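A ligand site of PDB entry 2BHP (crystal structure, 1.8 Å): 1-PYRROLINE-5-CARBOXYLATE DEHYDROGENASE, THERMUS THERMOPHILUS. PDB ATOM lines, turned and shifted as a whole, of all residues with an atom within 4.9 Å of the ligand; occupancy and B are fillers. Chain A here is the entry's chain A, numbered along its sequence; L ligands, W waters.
O of Gly 260 sits close to O11 of the ligand. Residues that only touch the ligand: Ile 180 (3.1 Å), Pro 182 (3.5 Å), Asn 184 (3.2 Å), Ile 189 (3.6 Å), Pro 208 (3.8 Å), Ala 209 (3.4 Å), Glu 241 (3.7 Å), Gly 244 (3.7 Å), Ala 245 (3.6 Å), Phe 258 (3.5 Å), Thr 259 (3.3 Å), Val 264 (3.4 Å), Glu 288 (3.4 Å), Gly 290 (3.0 Å), Phe 419 (3.2 Å), Leu 445 (3.7 Å) and Phe 485 (3.4 Å). Hydrophobic or aromatic side chains that line the ligand: Ile 180, Pro 182, Trp 183, Ile 189, Ala 209, Ala 245, Phe 258, Val 264, Phe 419, Leu 445 and Phe 485. Of the 36 residues printed, 27 come within 4 Å of the ligand. Along chain A the residues within 4 Å of the ligand span positions 180 to 485. The nearest printed residue that does not touch the ligand is Ile 268 (4.04 Å).
The side-chain amino group (NZ) of Lys 207 is in salt-bridge range of the side-chain carboxylate (OE1) of Glu 210 (3.6 Å). The backbone carbonyl oxygen of Ser 491 lies within hydrogen-bond range of the backbone NH of Thr 289, 3.0 Å away. The side-chain hydroxyl (OG) of Ser 261 lies within hydrogen-bond range of the backbone NH (N) of Val 264, at 3.4 Å. The backbone carbonyl oxygen (O) of Gly 238 sits at hydrogen-bond distance from the side-chain amino group (NZ) of Lys 207. O of Ala 181 sits close to N of Ala 209, 3.4 Å away. The backbone carbonyl oxygen (O) of Ile 180 is in hydrogen-bond range of the backbone NH (N) of Thr 259 (3.2 Å). N of Glu 288 lies within hydrogen-bond range of O of Phe 258 (3.0 Å). The side-chain hydroxyl of Ser 491 is in hydrogen-bond range of the backbone NH of Leu 445 (3.2 Å).
OE1 of Glu 210 is in hydrogen-bond range of O6 of the ligand (2.5 Å). The side-chain carboxylate of Glu 417 lies within hydrogen-bond range of an oxygen (O12) of the ligand, at 2.6 Å. A nitrogen (N7) of the ligand sits at hydrogen-bond distance from the backbone carbonyl oxygen of Thr 289, 2.6 Å away. N of Ser 261 is in hydrogen-bond range of O1 of the ligand, at 2.8 Å. The side-chain hydroxyl (OG) of Ser 261 sits at hydrogen-bond distance from an oxygen (O1) of the ligand (2.6 Å). NZ of Lys 207 lies within hydrogen-bond range of O6 of the ligand, at 2.7 Å. An oxygen (O8) of the ligand is in hydrogen-bond range of the indole nitrogen (NE1) of Trp 183, at 2.7 Å. The backbone carbonyl oxygen of Ala 181 is in hydrogen-bond range of an oxygen (O5) of the ligand (2.7 Å). The side-chain sulfur (SG) of Cys 322 sits close to an oxygen (O14) of the ligand (3.8 Å). An oxygen (O6) of the ligand lies close to the backbone NH (N) of Gly 240, 3.4 Å away.
Water W3 lies within hydrogen-bond range of N of Asn 184 (2.7 Å), O10 of the ligand (2.7 Å) and N of Trp 183 (3.0 Å). Water W4 lies within hydrogen-bond range of N2 of the ligand (2.8 Å) and OE2 of Glu 241 (3.1 Å). Water W6 lies within hydrogen-bond range of the side-chain carboxylate of Glu 241 (2.8 Å), a nitrogen (N3) of the ligand (2.9 Å) and the side-chain amino group of Lys 267 (3.4 Å). Water W1 lies within hydrogen-bond range of the side-chain carboxylate of Glu 288 (2.6 Å), the backbone carbonyl oxygen of Ser 491 (2.6 Å) and a nitrogen (N7) of the ligand (3.1 Å). Water W2 bridges the side-chain carboxylate of Glu 210 (2.8 Å) and an oxygen (O6) of the ligand (3.5 Å). Water W8 lies within hydrogen-bond range of OE2 of Glu 417, N of Leu 262, N of Gly 290 and O12 of the ligand.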
ATOM      1  N   ILE A 180      20.220 -21.094 -10.212  1.00  0.00           N
ATOM      2  CA  ILE A 180      19.715 -21.405  -8.880  1.00  0.00           C
ATOM      3  C   ILE A 180      19.326 -20.077  -8.266  1.00  0.00           C
ATOM      4  O   ILE A 180      20.175 -19.241  -8.001  1.00  0.00           O
ATOM      5  CB  ILE A 180      20.810 -22.116  -8.062  1.00  0.00           C
ATOM      6  CG1 ILE A 180      21.155 -23.442  -8.751  1.00  0.00           C
ATOM      7  CG2 ILE A 180      20.336 -22.347  -6.643  1.00  0.00           C
ATOM      8  CD1 ILE A 180      22.249 -24.241  -8.073  1.00  0.00           C
ATOM      9  N   ALA A 181      18.021 -19.907  -8.039  1.00  0.00           N
ATOM     10  CA  ALA A 181      17.457 -18.645  -7.564  1.00  0.00           C
ATOM     11  C   ALA A 181      16.935 -18.570  -6.139  1.00  0.00           C
ATOM     12  O   ALA A 181      16.609 -19.583  -5.521  1.00  0.00           O
ATOM     13  CB  ALA A 181      16.361 -18.211  -8.527  1.00  0.00           C
ATOM     14  N   PRO A 182      16.816 -17.341  -5.604  1.00  0.00           N
ATOM     15  CA  PRO A 182      16.338 -17.072  -4.248  1.00  0.00           C
ATOM     16  C   PRO A 182      14.827 -16.902  -4.182  1.00  0.00           C
ATOM     17  O   PRO A 182      14.160 -16.760  -5.219  1.00  0.00           O
ATOM     18  CB  PRO A 182      17.065 -15.785  -3.879  1.00  0.00           C
ATOM     19  CG  PRO A 182      16.970 -15.027  -5.175  1.00  0.00           C
ATOM     20  CD  PRO A 182      17.302 -16.092  -6.224  1.00  0.00           C
ATOM     21  N   TRP A 183      14.284 -16.896  -2.971  1.00  0.00           N
ATOM     22  CA  TRP A 183      12.835 -16.714  -2.797  1.00  0.00           C
ATOM     23  C   TRP A 183      12.393 -15.267  -2.630  1.00  0.00           C
ATOM     24  O   TRP A 183      11.211 -14.973  -2.761  1.00  0.00           O
ATOM     25  CB  TRP A 183      12.339 -17.516  -1.583  1.00  0.00           C
ATOM     26  CG  TRP A 183      13.112 -17.252  -0.314  1.00  0.00           C
ATOM     27  CD1 TRP A 183      14.116 -18.009   0.200  1.00  0.00           C
ATOM     28  CD2 TRP A 183      12.971 -16.124   0.571  1.00  0.00           C
ATOM     29  NE1 TRP A 183      14.617 -17.431   1.347  1.00  0.00           N
ATOM     30  CE2 TRP A 183      13.930 -16.267   1.592  1.00  0.00           C
ATOM     31  CE3 TRP A 183      12.127 -15.000   0.587  1.00  0.00           C
ATOM     32  CZ2 TRP A 183      14.084 -15.339   2.633  1.00  0.00           C
ATOM     33  CZ3 TRP A 183      12.271 -14.062   1.627  1.00  0.00           C
ATOM     34  CH2 TRP A 183      13.248 -14.251   2.631  1.00  0.00           C
ATOM     35  N   ASN A 184      13.330 -14.347  -2.373  1.00  0.00           N
ATOM     36  CA  ASN A 184      12.923 -12.965  -2.130  1.00  0.00           C
ATOM     37  C   ASN A 184      12.487 -12.144  -3.345  1.00  0.00           C
ATOM     38  O   ASN A 184      11.697 -11.224  -3.211  1.00  0.00           O
ATOM     39  CB  ASN A 184      13.997 -12.243  -1.313  1.00  0.00           C
ATOM     40  CG  ASN A 184      15.224 -11.901  -2.106  1.00  0.00           C
ATOM     41  OD1 ASN A 184      15.643 -12.644  -2.986  1.00  0.00           O
ATOM     42  ND2 ASN A 184      15.824 -10.749  -1.794  1.00  0.00           N
ATOM     43  N   ILE A 189      14.489 -11.853 -10.214  1.00  0.00           N
ATOM     44  CA  ILE A 189      15.808 -12.488 -10.313  1.00  0.00           C
ATOM     45  C   ILE A 189      15.782 -13.847 -10.997  1.00  0.00           C
ATOM     46  O   ILE A 189      16.710 -14.195 -11.734  1.00  0.00           O
ATOM     47  CB  ILE A 189      16.457 -12.580  -8.923  1.00  0.00           C
ATOM     48  CG1 ILE A 189      16.737 -11.163  -8.409  1.00  0.00           C
ATOM     49  CG2 ILE A 189      17.773 -13.360  -9.001  1.00  0.00           C
ATOM     50  CD1 ILE A 189      17.299 -11.107  -7.016  1.00  0.00           C
ATOM     51  N   LYS A 207      16.383 -23.777 -11.231  1.00  0.00           N
ATOM     52  CA  LYS A 207      16.021 -24.359  -9.948  1.00  0.00           C
ATOM     53  C   LYS A 207      15.485 -23.245  -9.044  1.00  0.00           C
ATOM     54  O   LYS A 207      16.266 -22.508  -8.433  1.00  0.00           O
ATOM     55  CB  LYS A 207      17.253 -25.016  -9.311  1.00  0.00           C
ATOM     56  CG  LYS A 207      16.970 -26.300  -8.527  1.00  0.00           C
ATOM     57  CD  LYS A 207      16.061 -26.043  -7.331  1.00  0.00           C
ATOM     58  CE  LYS A 207      16.761 -25.240  -6.243  1.00  0.00           C
ATOM     59  NZ  LYS A 207      15.878 -25.021  -5.073  1.00  0.00           N
ATOM     60  N   PRO A 208      14.159 -23.102  -8.954  1.00  0.00           N
ATOM     61  CA  PRO A 208      13.560 -22.056  -8.113  1.00  0.00           C
ATOM     62  C   PRO A 208      13.734 -22.362  -6.636  1.00  0.00           C
ATOM     63  O   PRO A 208      13.919 -23.524  -6.257  1.00  0.00           O
ATOM     64  CB  PRO A 208      12.097 -22.091  -8.520  1.00  0.00           C
ATOM     65  CG  PRO A 208      11.875 -23.566  -8.766  1.00  0.00           C
ATOM     66  CD  PRO A 208      13.107 -23.926  -9.589  1.00  0.00           C
ATOM     67  N   ALA A 209      13.664 -21.323  -5.806  1.00  0.00           N
ATOM     68  CA  ALA A 209      13.785 -21.506  -4.368  1.00  0.00           C
ATOM     69  C   ALA A 209      12.553 -22.274  -3.893  1.00  0.00           C
ATOM     70  O   ALA A 209      11.449 -22.089  -4.422  1.00  0.00           O
ATOM     71  CB  ALA A 209      13.875 -20.148  -3.666  1.00  0.00           C
ATOM     72  N   GLU A 210      12.733 -23.124  -2.885  1.00  0.00           N
ATOM     73  CA  GLU A 210      11.644 -23.928  -2.353  1.00  0.00           C
ATOM     74  C   GLU A 210      10.382 -23.151  -1.963  1.00  0.00           C
ATOM     75  O   GLU A 210       9.266 -23.614  -2.215  1.00  0.00           O
ATOM     76  CB  GLU A 210      12.152 -24.748  -1.153  1.00  0.00           C
ATOM     77  CG  GLU A 210      13.154 -25.826  -1.541  1.00  0.00           C
ATOM     78  CD  GLU A 210      14.607 -25.395  -1.393  1.00  0.00           C
ATOM     79  OE1 GLU A 210      14.923 -24.209  -1.662  1.00  0.00           O
ATOM     80  OE2 GLU A 210      15.443 -26.242  -1.018  1.00  0.00           O
ATOM     81  N   GLY A 238      12.925 -28.127  -6.628  1.00  0.00           N
ATOM     82  CA  GLY A 238      13.453 -29.212  -5.822  1.00  0.00           C
ATOM     83  C   GLY A 238      14.279 -28.672  -4.681  1.00  0.00           C
ATOM     84  O   GLY A 238      14.355 -27.458  -4.490  1.00  0.00           O
ATOM     85  N   VAL A 239      14.898 -29.562  -3.916  1.00  0.00           N
ATOM     86  CA  VAL A 239      15.715 -29.165  -2.766  1.00  0.00           C
ATOM     87  C   VAL A 239      17.113 -28.721  -3.178  1.00  0.00           C
ATOM     88  O   VAL A 239      17.826 -29.432  -3.889  1.00  0.00           O
ATOM     89  CB  VAL A 239      15.841 -30.338  -1.763  1.00  0.00           C
ATOM     90  CG1 VAL A 239      16.661 -29.897  -0.552  1.00  0.00           C
ATOM     91  CG2 VAL A 239      14.445 -30.786  -1.322  1.00  0.00           C
ATOM     92  N   GLY A 240      17.489 -27.527  -2.738  1.00  0.00           N
ATOM     93  CA  GLY A 240      18.792 -26.975  -3.080  1.00  0.00           C
ATOM     94  C   GLY A 240      19.980 -27.896  -2.856  1.00  0.00           C
ATOM     95  O   GLY A 240      20.745 -28.148  -3.786  1.00  0.00           O
ATOM     96  N   GLU A 241      20.131 -28.384  -1.629  1.00  0.00           N
ATOM     97  CA  GLU A 241      21.253 -29.264  -1.298  1.00  0.00           C
ATOM     98  C   GLU A 241      21.183 -30.612  -2.007  1.00  0.00           C
ATOM     99  O   GLU A 241      22.111 -31.416  -1.907  1.00  0.00           O
ATOM    100  CB  GLU A 241      21.324 -29.487   0.216  1.00  0.00           C
ATOM    101  CG  GLU A 241      21.401 -28.200   1.012  1.00  0.00           C
ATOM    102  CD  GLU A 241      21.503 -28.457   2.507  1.00  0.00           C
ATOM    103  OE1 GLU A 241      20.712 -29.263   3.035  1.00  0.00           O
ATOM    104  OE2 GLU A 241      22.382 -27.837   3.155  1.00  0.00           O
ATOM    105  N   GLY A 244      19.987 -29.182  -6.609  1.00  0.00           N
ATOM    106  CA  GLY A 244      20.795 -28.011  -6.890  1.00  0.00           C
ATOM    107  C   GLY A 244      22.283 -28.345  -6.851  1.00  0.00           C
ATOM    108  O   GLY A 244      23.027 -28.069  -7.800  1.00  0.00           O
ATOM    109  N   ALA A 245      22.712 -28.944  -5.756  1.00  0.00           N
ATOM    110  CA  ALA A 245      24.113 -29.322  -5.602  1.00  0.00           C
ATOM    111  C   ALA A 245      24.533 -30.338  -6.672  1.00  0.00           C
ATOM    112  O   ALA A 245      25.656 -30.299  -7.172  1.00  0.00           O
ATOM    113  CB  ALA A 245      24.353 -29.908  -4.220  1.00  0.00           C
ATOM    114  N   VAL A 248      25.318 -28.388  -9.768  1.00  0.00           N
ATOM    115  CA  VAL A 248      26.525 -27.585  -9.562  1.00  0.00           C
ATOM    116  C   VAL A 248      27.795 -28.429  -9.718  1.00  0.00           C
ATOM    117  O   VAL A 248      28.753 -27.994 -10.355  1.00  0.00           O
ATOM    118  CB  VAL A 248      26.547 -26.954  -8.144  1.00  0.00           C
ATOM    119  CG1 VAL A 248      27.930 -26.393  -7.832  1.00  0.00           C
ATOM    120  CG2 VAL A 248      25.502 -25.847  -8.052  1.00  0.00           C
ATOM    121  N   PHE A 258      24.064 -18.157  -9.900  1.00  0.00           N
ATOM    122  CA  PHE A 258      23.475 -18.233  -8.567  1.00  0.00           C
ATOM    123  C   PHE A 258      23.264 -16.915  -7.851  1.00  0.00           C
ATOM    124  O   PHE A 258      24.082 -16.013  -7.920  1.00  0.00           O
ATOM    125  CB  PHE A 258      24.361 -19.117  -7.682  1.00  0.00           C
ATOM    126  CG  PHE A 258      23.965 -19.130  -6.218  1.00  0.00           C
ATOM    127  CD1 PHE A 258      22.965 -19.987  -5.765  1.00  0.00           C
ATOM    128  CD2 PHE A 258      24.571 -18.260  -5.311  1.00  0.00           C
ATOM    129  CE1 PHE A 258      22.583 -19.984  -4.421  1.00  0.00           C
ATOM    130  CE2 PHE A 258      24.202 -18.253  -3.964  1.00  0.00           C
ATOM    131  CZ  PHE A 258      23.197 -19.116  -3.518  1.00  0.00           C
ATOM    132  N   THR A 259      22.141 -16.828  -7.156  1.00  0.00           N
ATOM    133  CA  THR A 259      21.835 -15.650  -6.355  1.00  0.00           C
ATOM    134  C   THR A 259      21.256 -16.225  -5.063  1.00  0.00           C
ATOM    135  O   THR A 259      20.283 -16.977  -5.094  1.00  0.00           O
ATOM    136  CB  THR A 259      20.824 -14.730  -7.039  1.00  0.00           C
ATOM    137  OG1 THR A 259      21.404 -14.193  -8.243  1.00  0.00           O
ATOM    138  CG2 THR A 259      20.474 -13.583  -6.130  1.00  0.00           C
ATOM    139  N   GLY A 260      21.878 -15.900  -3.952  1.00  0.00           N
ATOM    140  CA  GLY A 260      21.404 -16.429  -2.689  1.00  0.00           C
ATOM    141  C   GLY A 260      22.321 -16.061  -1.533  1.00  0.00           C
ATOM    142  O   GLY A 260      23.033 -15.072  -1.595  1.00  0.00           O
ATOM    143  N   SER A 261      22.287 -16.872  -0.472  1.00  0.00           N
ATOM    144  CA  SER A 261      23.090 -16.600   0.715  1.00  0.00           C
ATOM    145  C   SER A 261      24.577 -16.822   0.494  1.00  0.00           C
ATOM    146  O   SER A 261      24.993 -17.580  -0.387  1.00  0.00           O
ATOM    147  CB  SER A 261      22.633 -17.484   1.874  1.00  0.00           C
ATOM    148  OG  SER A 261      22.934 -18.849   1.611  1.00  0.00           O
ATOM    149  N   LEU A 262      25.387 -16.146   1.308  1.00  0.00           N
ATOM    150  CA  LEU A 262      26.829 -16.278   1.224  1.00  0.00           C
ATOM    151  C   LEU A 262      27.223 -17.725   1.554  1.00  0.00           C
ATOM    152  O   LEU A 262      28.121 -18.296   0.929  1.00  0.00           O
ATOM    153  CB  LEU A 262      27.522 -15.324   2.194  1.00  0.00           C
ATOM    154  CG  LEU A 262      29.036 -15.486   2.348  1.00  0.00           C
ATOM    155  CD1 LEU A 262      29.725 -15.349   0.991  1.00  0.00           C
ATOM    156  CD2 LEU A 262      29.555 -14.438   3.317  1.00  0.00           C
ATOM    157  N   VAL A 264      25.744 -20.592   0.985  1.00  0.00           N
ATOM    158  CA  VAL A 264      25.588 -21.450  -0.183  1.00  0.00           C
ATOM    159  C   VAL A 264      26.503 -21.011  -1.324  1.00  0.00           C
ATOM    160  O   VAL A 264      27.096 -21.838  -2.013  1.00  0.00           O
ATOM    161  CB  VAL A 264      24.126 -21.456  -0.671  1.00  0.00           C
ATOM    162  CG1 VAL A 264      24.014 -22.200  -2.001  1.00  0.00           C
ATOM    163  CG2 VAL A 264      23.245 -22.148   0.370  1.00  0.00           C
ATOM    164  N   LYS A 267      29.988 -22.454  -1.076  1.00  0.00           N
ATOM    165  CA  LYS A 267      30.063 -23.870  -1.447  1.00  0.00           C
ATOM    166  C   LYS A 267      29.995 -24.032  -2.962  1.00  0.00           C
ATOM    167  O   LYS A 267      30.717 -24.838  -3.547  1.00  0.00           O
ATOM    168  CB  LYS A 267      28.915 -24.657  -0.808  1.00  0.00           C
ATOM    169  CG  LYS A 267      28.994 -24.723   0.715  1.00  0.00           C
ATOM    170  CD  LYS A 267      27.766 -25.394   1.308  1.00  0.00           C
ATOM    171  CE  LYS A 267      27.898 -25.499   2.817  1.00  0.00           C
ATOM    172  NZ  LYS A 267      26.705 -26.150   3.430  1.00  0.00           N
ATOM    173  N   ILE A 268      29.126 -23.255  -3.601  1.00  0.00           N
ATOM    174  CA  ILE A 268      28.977 -23.313  -5.039  1.00  0.00           C
ATOM    175  C   ILE A 268      30.241 -22.847  -5.771  1.00  0.00           C
ATOM    176  O   ILE A 268      30.677 -23.471  -6.729  1.00  0.00           O
ATOM    177  CB  ILE A 268      27.776 -22.469  -5.506  1.00  0.00           C
ATOM    178  CG1 ILE A 268      26.473 -23.153  -5.070  1.00  0.00           C
ATOM    179  CG2 ILE A 268      27.812 -22.276  -7.017  1.00  0.00           C
ATOM    180  CD1 ILE A 268      25.215 -22.411  -5.478  1.00  0.00           C
ATOM    181  N   GLU A 288      25.939 -14.125  -6.570  1.00  0.00           N
ATOM    182  CA  GLU A 288      25.604 -12.831  -6.016  1.00  0.00           C
ATOM    183  C   GLU A 288      25.044 -13.228  -4.653  1.00  0.00           C
ATOM    184  O   GLU A 288      23.970 -13.835  -4.544  1.00  0.00           O
ATOM    185  CB  GLU A 288      24.639 -12.136  -6.956  1.00  0.00           C
ATOM    186  CG  GLU A 288      25.287 -12.021  -8.370  1.00  0.00           C
ATOM    187  CD  GLU A 288      26.663 -11.346  -8.331  1.00  0.00           C
ATOM    188  OE1 GLU A 288      27.579 -11.724  -9.107  1.00  0.00           O
ATOM    189  OE2 GLU A 288      26.839 -10.413  -7.532  1.00  0.00           O
ATOM    190  N   THR A 289      25.772 -12.853  -3.617  1.00  0.00           N
ATOM    191  CA  THR A 289      25.403 -13.201  -2.265  1.00  0.00           C
ATOM    192  C   THR A 289      24.809 -12.035  -1.482  1.00  0.00           C
ATOM    193  O   THR A 289      24.382 -11.043  -2.061  1.00  0.00           O
ATOM    194  CB  THR A 289      26.640 -13.757  -1.557  1.00  0.00           C
ATOM    195  OG1 THR A 289      27.760 -12.911  -1.845  1.00  0.00           O
ATOM    196  CG2 THR A 289      26.941 -15.164  -2.070  1.00  0.00           C
ATOM    197  N   GLY A 290      24.756 -12.184  -0.167  1.00  0.00           N
ATOM    198  CA  GLY A 290      24.156 -11.143   0.650  1.00  0.00           C
ATOM    199  C   GLY A 290      24.962  -9.897   0.891  1.00  0.00           C
ATOM    200  O   GLY A 290      25.965  -9.629   0.219  1.00  0.00           O
ATOM    201  N   GLY A 291      24.508  -9.125   1.853  1.00  0.00           N
ATOM    202  CA  GLY A 291      25.195  -7.894   2.205  1.00  0.00           C
ATOM    203  C   GLY A 291      24.793  -7.485   3.601  1.00  0.00           C
ATOM    204  O   GLY A 291      23.920  -8.102   4.223  1.00  0.00           O
ATOM    205  N   CYS A 322      18.688  -8.203  -0.256  1.00  0.00           N
ATOM    206  CA  CYS A 322      20.131  -8.192  -0.173  1.00  0.00           C
ATOM    207  C   CYS A 322      20.607  -6.749  -0.137  1.00  0.00           C
ATOM    208  O   CYS A 322      21.739  -6.469   0.239  1.00  0.00           O
ATOM    209  CB  CYS A 322      20.740  -8.871  -1.388  1.00  0.00           C
ATOM    210  SG  CYS A 322      20.430  -7.979  -2.933  1.00  0.00           S
ATOM    211  N   GLN A 368      12.769 -18.910   8.634  1.00  0.00           N
ATOM    212  CA  GLN A 368      13.274 -17.541   8.543  1.00  0.00           C
ATOM    213  C   GLN A 368      12.857 -16.813   9.817  1.00  0.00           C
ATOM    214  O   GLN A 368      13.632 -16.048  10.381  1.00  0.00           O
ATOM    215  CB  GLN A 368      12.724 -16.825   7.311  1.00  0.00           C
ATOM    216  CG  GLN A 368      13.491 -17.132   6.042  1.00  0.00           C
ATOM    217  CD  GLN A 368      14.975 -16.845   6.189  1.00  0.00           C
ATOM    218  OE1 GLN A 368      15.807 -17.752   6.046  1.00  0.00           O
ATOM    219  NE2 GLN A 368      15.305 -15.600   6.486  1.00  0.00           N
ATOM    220  N   GLU A 417      24.288 -10.928   8.152  1.00  0.00           N
ATOM    221  CA  GLU A 417      23.040 -10.633   7.464  1.00  0.00           C
ATOM    222  C   GLU A 417      21.875 -11.347   8.138  1.00  0.00           C
ATOM    223  O   GLU A 417      21.788 -12.580   8.098  1.00  0.00           O
ATOM    224  CB  GLU A 417      23.135 -11.073   5.991  1.00  0.00           C
ATOM    225  CG  GLU A 417      21.939 -10.651   5.155  1.00  0.00           C
ATOM    226  CD  GLU A 417      22.061 -11.077   3.712  1.00  0.00           C
ATOM    227  OE1 GLU A 417      21.786 -10.247   2.820  1.00  0.00           O
ATOM    228  OE2 GLU A 417      22.419 -12.252   3.459  1.00  0.00           O
ATOM    229  N   PHE A 419      18.537 -10.510   7.458  1.00  0.00           N
ATOM    230  CA  PHE A 419      17.503 -10.665   6.454  1.00  0.00           C
ATOM    231  C   PHE A 419      16.090 -10.615   7.041  1.00  0.00           C
ATOM    232  O   PHE A 419      15.220 -11.408   6.669  1.00  0.00           O
ATOM    233  CB  PHE A 419      17.702 -11.983   5.689  1.00  0.00           C
ATOM    234  CG  PHE A 419      17.553 -11.841   4.202  1.00  0.00           C
ATOM    235  CD1 PHE A 419      16.522 -12.491   3.527  1.00  0.00           C
ATOM    236  CD2 PHE A 419      18.417 -11.030   3.471  1.00  0.00           C
ATOM    237  CE1 PHE A 419      16.354 -12.340   2.144  1.00  0.00           C
ATOM    238  CE2 PHE A 419      18.258 -10.868   2.102  1.00  0.00           C
ATOM    239  CZ  PHE A 419      17.227 -11.519   1.427  1.00  0.00           C
ATOM    240  N   LEU A 445      27.667  -4.712  -0.907  1.00  0.00           N
ATOM    241  CA  LEU A 445      26.597  -4.686  -1.909  1.00  0.00           C
ATOM    242  C   LEU A 445      25.985  -3.306  -2.110  1.00  0.00           C
ATOM    243  O   LEU A 445      26.237  -2.674  -3.141  1.00  0.00           O
ATOM    244  CB  LEU A 445      25.513  -5.712  -1.553  1.00  0.00           C
ATOM    245  CG  LEU A 445      24.466  -6.010  -2.632  1.00  0.00           C
ATOM    246  CD1 LEU A 445      25.126  -6.156  -3.997  1.00  0.00           C
ATOM    247  CD2 LEU A 445      23.713  -7.295  -2.262  1.00  0.00           C
ATOM    248  N   PHE A 485      23.398  -3.665 -11.142  1.00  0.00           N
ATOM    249  CA  PHE A 485      23.362  -4.220  -9.792  1.00  0.00           C
ATOM    250  C   PHE A 485      24.306  -5.389  -9.477  1.00  0.00           C
ATOM    251  O   PHE A 485      24.277  -6.423 -10.138  1.00  0.00           O
ATOM    252  CB  PHE A 485      21.924  -4.628  -9.458  1.00  0.00           C
ATOM    253  CG  PHE A 485      21.708  -4.930  -8.007  1.00  0.00           C
ATOM    254  CD1 PHE A 485      21.641  -3.902  -7.071  1.00  0.00           C
ATOM    255  CD2 PHE A 485      21.595  -6.246  -7.568  1.00  0.00           C
ATOM    256  CE1 PHE A 485      21.466  -4.175  -5.710  1.00  0.00           C
ATOM    257  CE2 PHE A 485      21.417  -6.533  -6.209  1.00  0.00           C
ATOM    258  CZ  PHE A 485      21.357  -5.499  -5.282  1.00  0.00           C
ATOM    259  N   SER A 491      29.935 -10.077  -1.153  1.00  0.00           N
ATOM    260  CA  SER A 491      28.587  -9.837  -1.652  1.00  0.00           C
ATOM    261  C   SER A 491      28.497 -10.463  -3.048  1.00  0.00           C
ATOM    262  O   SER A 491      27.459 -10.396  -3.705  1.00  0.00           O
ATOM    263  CB  SER A 491      28.278  -8.338  -1.720  1.00  0.00           C
ATOM    264  OG  SER A 491      27.992  -7.850  -0.413  1.00  0.00           O
HETATM  265  P1  LIG L   1      19.823 -19.668  -0.089  1.00  0.00           P
HETATM  266  O1  LIG L   1      21.277 -19.503  -0.349  1.00  0.00           O
HETATM  267  O2  LIG L   1      19.526 -20.324   1.215  1.00  0.00           O
HETATM  268  O3  LIG L   1      19.210 -20.530  -1.279  1.00  0.00           O
HETATM  269  C1  LIG L   1      19.286 -19.993  -2.611  1.00  0.00           C
HETATM  270  C2  LIG L   1      18.938 -21.064  -3.634  1.00  0.00           C
HETATM  271  O4  LIG L   1      19.952 -22.094  -3.557  1.00  0.00           O
HETATM  272  C3  LIG L   1      17.585 -21.798  -3.483  1.00  0.00           C
HETATM  273  O5  LIG L   1      17.142 -22.125  -4.812  1.00  0.00           O
HETATM  274  C4  LIG L   1      17.997 -23.088  -2.710  1.00  0.00           C
HETATM  275  O6  LIG L   1      17.111 -24.166  -2.871  1.00  0.00           O
HETATM  276  C5  LIG L   1      19.385 -23.347  -3.325  1.00  0.00           C
HETATM  277  N1  LIG L   1      20.364 -24.057  -2.495  1.00  0.00           N
HETATM  278  C6  LIG L   1      20.441 -24.215  -1.136  1.00  0.00           C
HETATM  279  N2  LIG L   1      21.477 -24.925  -0.737  1.00  0.00           N
HETATM  280  C7  LIG L   1      22.116 -25.251  -1.916  1.00  0.00           C
HETATM  281  C8  LIG L   1      23.298 -25.997  -2.226  1.00  0.00           C
HETATM  282  N3  LIG L   1      24.085 -26.573  -1.305  1.00  0.00           N
HETATM  283  N4  LIG L   1      23.657 -26.135  -3.547  1.00  0.00           N
HETATM  284  C9  LIG L   1      22.893 -25.574  -4.512  1.00  0.00           C
HETATM  285  N5  LIG L   1      21.764 -24.847  -4.345  1.00  0.00           N
HETATM  286  C10 LIG L   1      21.436 -24.737  -3.020  1.00  0.00           C
HETATM  287  O7  LIG L   1      19.095 -18.242  -0.146  1.00  0.00           O
HETATM  288  P2  LIG L   1      17.618 -17.708   0.058  1.00  0.00           P
HETATM  289  O8  LIG L   1      17.273 -17.773   1.507  1.00  0.00           O
HETATM  290  O9  LIG L   1      16.751 -18.375  -0.956  1.00  0.00           O
HETATM  291  O10 LIG L   1      17.854 -16.208  -0.447  1.00  0.00           O
HETATM  292  C11 LIG L   1      18.205 -15.166   0.499  1.00  0.00           C
HETATM  293  C12 LIG L   1      19.680 -14.869   0.332  1.00  0.00           C
HETATM  294  O11 LIG L   1      19.907 -14.446  -1.039  1.00  0.00           O
HETATM  295  C13 LIG L   1      20.200 -13.727   1.223  1.00  0.00           C
HETATM  296  O12 LIG L   1      21.494 -13.980   1.752  1.00  0.00           O
HETATM  297  C14 LIG L   1      20.306 -12.553   0.238  1.00  0.00           C
HETATM  298  O13 LIG L   1      21.236 -11.562   0.597  1.00  0.00           O
HETATM  299  C15 LIG L   1      20.645 -13.277  -1.064  1.00  0.00           C
HETATM  300  N6  LIG L   1      20.254 -12.500  -2.284  1.00  0.00           N
HETATM  301  C16 LIG L   1      21.277 -11.922  -2.977  1.00  0.00           C
HETATM  302  C17 LIG L   1      20.994 -11.032  -4.027  1.00  0.00           C
HETATM  303  C18 LIG L   1      22.079 -10.354  -4.838  1.00  0.00           C
HETATM  304  O14 LIG L   1      21.776  -9.861  -5.936  1.00  0.00           O
HETATM  305  N7  LIG L   1      23.310 -10.301  -4.336  1.00  0.00           N
HETATM  306  C19 LIG L   1      19.628 -10.791  -4.347  1.00  0.00           C
HETATM  307  C20 LIG L   1      18.602 -11.556  -3.740  1.00  0.00           C
HETATM  308  C21 LIG L   1      18.924 -12.403  -2.692  1.00  0.00           C
HETATM  309  O   HOH W   1      25.971  -9.129  -5.478  1.00  0.00           O
HETATM  310  O   HOH W   2      17.569 -25.180   0.416  1.00  0.00           O
HETATM  311  O   HOH W   3      15.449 -14.976  -0.910  1.00  0.00           O
HETATM  312  O   HOH W   4      21.465 -25.033   2.051  1.00  0.00           O
HETATM  313  O   HOH W   5      21.656  -9.826  -8.502  1.00  0.00           O
HETATM  314  O   HOH W   6      23.863 -26.118   1.506  1.00  0.00           O
HETATM  315  O   HOH W   7      15.789 -20.920  -0.689  1.00  0.00           O
HETATM  316  O   HOH W   8      24.748 -13.654   2.971  1.00  0.00           O
